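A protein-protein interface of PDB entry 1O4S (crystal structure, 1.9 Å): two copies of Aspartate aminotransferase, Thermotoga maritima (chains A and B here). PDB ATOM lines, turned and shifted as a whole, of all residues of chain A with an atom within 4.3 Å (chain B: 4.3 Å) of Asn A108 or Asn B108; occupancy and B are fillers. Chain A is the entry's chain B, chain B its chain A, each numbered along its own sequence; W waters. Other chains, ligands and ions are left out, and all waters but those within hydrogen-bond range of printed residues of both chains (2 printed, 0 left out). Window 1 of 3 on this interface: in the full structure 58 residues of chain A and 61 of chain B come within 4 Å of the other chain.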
ATOM      1  N   THR A 107       5.844  -4.324 -14.543  1.00  0.00           N
ATOM      2  CA  THR A 107       5.544  -2.942 -14.240  1.00  0.00           C
ATOM      3  C   THR A 107       5.487  -2.678 -12.742  1.00  0.00           C
ATOM      4  O   THR A 107       5.438  -3.593 -11.922  1.00  0.00           O
ATOM      5  CB  THR A 107       4.132  -2.615 -14.826  1.00  0.00           C
ATOM      6  OG1 THR A 107       3.139  -3.462 -14.201  1.00  0.00           O
ATOM      7  CG2 THR A 107       4.019  -2.927 -16.365  1.00  0.00           C
ATOM      8  N   ASN A 108       5.481  -1.413 -12.379  1.00  0.00           N
ATOM      9  CA  ASN A 108       5.391  -0.994 -10.986  1.00  0.00           C
ATOM     10  C   ASN A 108       3.949  -1.092 -10.509  1.00  0.00           C
ATOM     11  O   ASN A 108       3.180  -0.127 -10.576  1.00  0.00           O
ATOM     12  CB  ASN A 108       5.885   0.455 -10.830  1.00  0.00           C
ATOM     13  CG  ASN A 108       7.387   0.585 -10.967  1.00  0.00           C
ATOM     14  OD1 ASN A 108       8.102   0.159 -10.087  1.00  0.00           O
ATOM     15  ND2 ASN A 108       7.866   1.217 -12.049  1.00  0.00           N
ATOM     16  N   GLY A 109       3.638  -2.235  -9.949  1.00  0.00           N
ATOM     17  CA  GLY A 109       2.278  -2.648  -9.661  1.00  0.00           C
ATOM     18  C   GLY A 109       1.451  -2.869 -10.915  1.00  0.00           C
ATOM     19  O   GLY A 109       1.848  -2.526 -12.057  1.00  0.00           O
ATOM     20  N   GLN A 112       0.680   0.647 -12.836  1.00  0.00           N
ATOM     21  CA  GLN A 112       1.420   1.071 -13.995  1.00  0.00           C
ATOM     22  C   GLN A 112       1.123   0.176 -15.197  1.00  0.00           C
ATOM     23  O   GLN A 112       1.162   0.659 -16.315  1.00  0.00           O
ATOM     24  CB  GLN A 112       2.937   1.150 -13.699  1.00  0.00           C
ATOM     25  CG  GLN A 112       3.729   1.849 -14.840  1.00  0.00           C
ATOM     26  CD  GLN A 112       5.255   1.805 -14.700  1.00  0.00           C
ATOM     27  OE1 GLN A 112       5.822   0.954 -13.999  1.00  0.00           O
ATOM     28  NE2 GLN A 112       5.920   2.735 -15.379  1.00  0.00           N
ATOM     29  N   ARG A 254       5.652  -3.014  -5.346  1.00  0.00           N
ATOM     30  CA  ARG A 254       5.238  -2.472  -6.643  1.00  0.00           C
ATOM     31  C   ARG A 254       5.680  -3.348  -7.802  1.00  0.00           C
ATOM     32  O   ARG A 254       6.510  -2.907  -8.595  1.00  0.00           O
ATOM     33  CB  ARG A 254       5.725  -1.020  -6.856  1.00  0.00           C
ATOM     34  CG  ARG A 254       5.740  -0.134  -5.603  1.00  0.00           C
ATOM     35  CD  ARG A 254       4.396   0.170  -4.969  1.00  0.00           C
ATOM     36  NE  ARG A 254       3.404   0.598  -5.945  1.00  0.00           N
ATOM     37  CZ  ARG A 254       2.336  -0.089  -6.345  1.00  0.00           C
ATOM     38  NH1 ARG A 254       2.055  -1.281  -5.846  1.00  0.00           N
ATOM     39  NH2 ARG A 254       1.534   0.431  -7.267  1.00  0.00           N
ATOM     40  N   GLN A 272       7.047   1.794 -20.756  1.00  0.00           N
ATOM     41  CA  GLN A 272       7.706   1.416 -19.504  1.00  0.00           C
ATOM     42  C   GLN A 272       9.111   1.938 -19.524  1.00  0.00           C
ATOM     43  O   GLN A 272       9.580   2.553 -18.574  1.00  0.00           O
ATOM     44  CB  GLN A 272       7.707  -0.122 -19.324  1.00  0.00           C
ATOM     45  CG  GLN A 272       8.302  -0.640 -17.987  1.00  0.00           C
ATOM     46  CD  GLN A 272       7.450  -0.335 -16.782  1.00  0.00           C
ATOM     47  OE1 GLN A 272       6.246  -0.235 -16.887  1.00  0.00           O
ATOM     48  NE2 GLN A 272       8.073  -0.241 -15.629  1.00  0.00           N
ATOM     49  N   THR A 276       9.618   5.082 -16.491  1.00  0.00           N
ATOM     50  CA  THR A 276      10.290   4.676 -15.260  1.00  0.00           C
ATOM     51  C   THR A 276      11.494   3.795 -15.517  1.00  0.00           C
ATOM     52  O   THR A 276      12.258   3.522 -14.596  1.00  0.00           O
ATOM     53  CB  THR A 276       9.354   3.845 -14.335  1.00  0.00           C
ATOM     54  OG1 THR A 276       8.868   2.679 -15.034  1.00  0.00           O
ATOM     55  CG2 THR A 276       8.153   4.606 -13.954  1.00  0.00           C
ATOM     56  N   ILE A 279      11.741  -1.837 -13.363  1.00  0.00           N
ATOM     57  CA  ILE A 279      11.362  -1.735 -11.946  1.00  0.00           C
ATOM     58  C   ILE A 279      12.521  -2.187 -11.070  1.00  0.00           C
ATOM     59  O   ILE A 279      13.450  -2.846 -11.499  1.00  0.00           O
ATOM     60  CB  ILE A 279      10.043  -2.485 -11.614  1.00  0.00           C
ATOM     61  CG1 ILE A 279      10.232  -3.999 -11.463  1.00  0.00           C
ATOM     62  CG2 ILE A 279       8.972  -2.198 -12.665  1.00  0.00           C
ATOM     63  CD1 ILE A 279       9.036  -4.733 -10.801  1.00  0.00           C
ATOM     64  N   THR B 107      10.212   9.528  -6.698  1.00  0.00           N
ATOM     65  CA  THR B 107       9.798   8.908  -7.958  1.00  0.00           C
ATOM     66  C   THR B 107      10.706   7.728  -8.348  1.00  0.00           C
ATOM     67  O   THR B 107      11.788   7.598  -7.824  1.00  0.00           O
ATOM     68  CB  THR B 107       9.920   9.985  -9.146  1.00  0.00           C
ATOM     69  OG1 THR B 107      11.305  10.389  -9.339  1.00  0.00           O
ATOM     70  CG2 THR B 107       9.110  11.279  -8.916  1.00  0.00           C
ATOM     71  N   ASN B 108      10.281   6.932  -9.319  1.00  0.00           N
ATOM     72  CA  ASN B 108      11.041   5.747  -9.800  1.00  0.00           C
ATOM     73  C   ASN B 108      12.146   6.213 -10.737  1.00  0.00           C
ATOM     74  O   ASN B 108      11.995   6.268 -11.969  1.00  0.00           O
ATOM     75  CB  ASN B 108      10.140   4.738 -10.494  1.00  0.00           C
ATOM     76  CG  ASN B 108       9.231   4.015  -9.558  1.00  0.00           C
ATOM     77  OD1 ASN B 108       9.690   3.183  -8.775  1.00  0.00           O
ATOM     78  ND2 ASN B 108       7.903   4.284  -9.653  1.00  0.00           N
ATOM     79  N   GLY B 109      13.266   6.551 -10.106  1.00  0.00           N
ATOM     80  CA  GLY B 109      14.401   7.170 -10.749  1.00  0.00           C
ATOM     81  C   GLY B 109      14.113   8.635 -11.058  1.00  0.00           C
ATOM     82  O   GLY B 109      12.963   9.125 -10.950  1.00  0.00           O
ATOM     83  N   GLN B 112      11.475   8.948 -13.953  1.00  0.00           N
ATOM     84  CA  GLN B 112      10.071   9.210 -13.724  1.00  0.00           C
ATOM     85  C   GLN B 112       9.791  10.644 -13.259  1.00  0.00           C
ATOM     86  O   GLN B 112       8.726  11.189 -13.543  1.00  0.00           O
ATOM     87  CB  GLN B 112       9.439   8.193 -12.781  1.00  0.00           C
ATOM     88  CG  GLN B 112       7.932   8.386 -12.645  1.00  0.00           C
ATOM     89  CD  GLN B 112       7.252   7.454 -11.634  1.00  0.00           C
ATOM     90  OE1 GLN B 112       7.863   7.040 -10.646  1.00  0.00           O
ATOM     91  NE2 GLN B 112       5.970   7.170 -11.871  1.00  0.00           N
ATOM     92  N   ARG B 254      15.824   2.422  -8.429  1.00  0.00           N
ATOM     93  CA  ARG B 254      14.834   3.303  -9.053  1.00  0.00           C
ATOM     94  C   ARG B 254      14.290   4.316  -8.022  1.00  0.00           C
ATOM     95  O   ARG B 254      13.100   4.316  -7.671  1.00  0.00           O
ATOM     96  CB  ARG B 254      13.701   2.536  -9.744  1.00  0.00           C
ATOM     97  CG  ARG B 254      14.052   1.250 -10.457  1.00  0.00           C
ATOM     98  CD  ARG B 254      15.090   1.391 -11.602  1.00  0.00           C
ATOM     99  NE  ARG B 254      14.670   2.460 -12.508  1.00  0.00           N
ATOM    100  CZ  ARG B 254      15.299   3.598 -12.712  1.00  0.00           C
ATOM    101  NH1 ARG B 254      16.439   3.877 -12.117  1.00  0.00           N
ATOM    102  NH2 ARG B 254      14.757   4.493 -13.516  1.00  0.00           N
ATOM    103  N   GLN B 272       2.197  10.937 -10.122  1.00  0.00           N
ATOM    104  CA  GLN B 272       2.860   9.801  -9.445  1.00  0.00           C
ATOM    105  C   GLN B 272       1.835   8.886  -8.877  1.00  0.00           C
ATOM    106  O   GLN B 272       1.886   7.691  -9.018  1.00  0.00           O
ATOM    107  CB  GLN B 272       3.746  10.307  -8.328  1.00  0.00           C
ATOM    108  CG  GLN B 272       4.548   9.233  -7.597  1.00  0.00           C
ATOM    109  CD  GLN B 272       5.659   8.690  -8.436  1.00  0.00           C
ATOM    110  OE1 GLN B 272       6.194   9.396  -9.305  1.00  0.00           O
ATOM    111  NE2 GLN B 272       6.044   7.468  -8.176  1.00  0.00           N
ATOM    112  N   THR B 276       2.052   5.107 -11.037  1.00  0.00           N
ATOM    113  CA  THR B 276       2.710   3.997 -10.342  1.00  0.00           C
ATOM    114  C   THR B 276       2.313   3.883  -8.879  1.00  0.00           C
ATOM    115  O   THR B 276       2.668   2.928  -8.196  1.00  0.00           O
ATOM    116  CB  THR B 276       4.204   4.155 -10.383  1.00  0.00           C
ATOM    117  OG1 THR B 276       4.585   5.421  -9.826  1.00  0.00           O
ATOM    118  CG2 THR B 276       4.725   4.143 -11.819  1.00  0.00           C
ATOM    119  N   ILE B 279       6.661   4.584  -4.656  1.00  0.00           N
ATOM    120  CA  ILE B 279       7.740   3.718  -5.087  1.00  0.00           C
ATOM    121  C   ILE B 279       7.997   2.601  -4.071  1.00  0.00           C
ATOM    122  O   ILE B 279       7.596   2.666  -2.923  1.00  0.00           O
ATOM    123  CB  ILE B 279       9.044   4.486  -5.442  1.00  0.00           C
ATOM    124  CG1 ILE B 279       9.807   4.976  -4.207  1.00  0.00           C
ATOM    125  CG2 ILE B 279       8.771   5.641  -6.430  1.00  0.00           C
ATOM    126  CD1 ILE B 279      11.255   5.285  -4.528  1.00  0.00           C
HETATM  127  O   HOH W   1      10.760   0.473  -9.480  1.00  0.00           O
HETATM  128  O   HOH W   2       8.527   1.305  -7.300  1.00  0.00           O
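Water W2 lies within hydrogen-bond range of OD1 of Asn B108 and OD1 of Asn A108. Water W1 bridges OD1 of Asn A108 (2.7 Å) and OD1 of Asn B108 (3.0 Å).
The guanidinium group (NH2) of Arg B254 sits at hydrogen-bond distance from the backbone carbonyl oxygen (O) of Thr A276 (2.9 Å). The guanidinium group (NH2) of Arg A254 sits at hydrogen-bond distance from the backbone carbonyl oxygen (O) of Thr B276.
Asn B108 touches its own counterpart, Asn A108. Asn A108 touches Thr B276, and with the chains exchanged Thr A276 touches Asn B108. Gln A112 touches Thr B276, and with the chains exchanged Thr A276 touches Gln B112. Arg A254 touches Ile B279, and with the chains exchanged Ile A279 touches Arg B254. Of the 9 pairs that touch across the chains among the printed residues, 9 have their exchanged pair printed and touching as well.
The backbone NH (N) of Gly B109 sits close to the backbone carbonyl oxygen (O) of Arg B254, at 3.3 Å. The side-chain amide oxygen (OE1) of Gln B112 is in hydrogen-bond range of the side-chain amide nitrogen (NE2) of Gln B272 (3.1 Å). ND2 of Asn A108 is in hydrogen-bond range of OG1 of Thr A276 (3.5 Å). N of Gly A109 lies close to O of Arg A254, at 3.2 Å. The side-chain amide nitrogen of Gln A272 sits at hydrogen-bond distance from the side-chain amide oxygen of Gln A112 (3.0 Å). OG1 of Thr A276 is in hydrogen-bond range of NE2 of Gln A112 (3.0 Å).
Of the 8 printed residues of chain A, 5 touch a printed residue of chain B. Among the printed residues, 9 pairs touch across the chains. Among the printed residues, no Asp or Glu carboxylate lies within 4 Å of a Lys or Arg side-chain nitrogen of the other chain.
Among the printed residues, merely in contact across the chains: Asn A108 with Asn B108 (3.7 Å), Asn A108 with Thr B276 (3.9 Å), Gln A112 with Thr B276 (3.7 Å), Arg A254 with Ile B279 (3.9 Å), Thr A276 with Asn B108 (3.8 Å), Thr A276 with Gln B112 (3.8 Å) and Ile A279 with Arg B254 (3.8 Å).
Thr A107 touches none of the printed residues of chain B. Asn A108 touches just these residues of chain B: Asn B108 (3.7 Å) and Thr B276 (3.9 Å). Printed residues of chain B within 4 Å of Thr A276: Asn B108 (3.8 Å), Gln B112 (3.8 Å) and Arg B254 (2.9 Å). Printed residues of chain B within 4 Å of Ile A279: Arg B254. Thr B107 touches none of the printed residues of chain A. Of the printed residues of chain A, Asn B108 touches Asn A108 and Thr A276. Of the printed residues of chain A, Gln B112 touches Thr A276 (3.8 Å). Printed residues of chain A within 4 Å of Arg B254: Thr A276 (2.9 Å) and Ile A279 (3.8 Å). Printed residues of chain A within 4 Å of Thr B276: Asn A108, Gln A112 and Arg A254. The nearest printed residue of chain A that does not touch Asn B108 is Gln A112 (5.9 Å). The nearest printed residue of chain B that does not touch Gln A112 is Gln B112 (5.7 Å).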
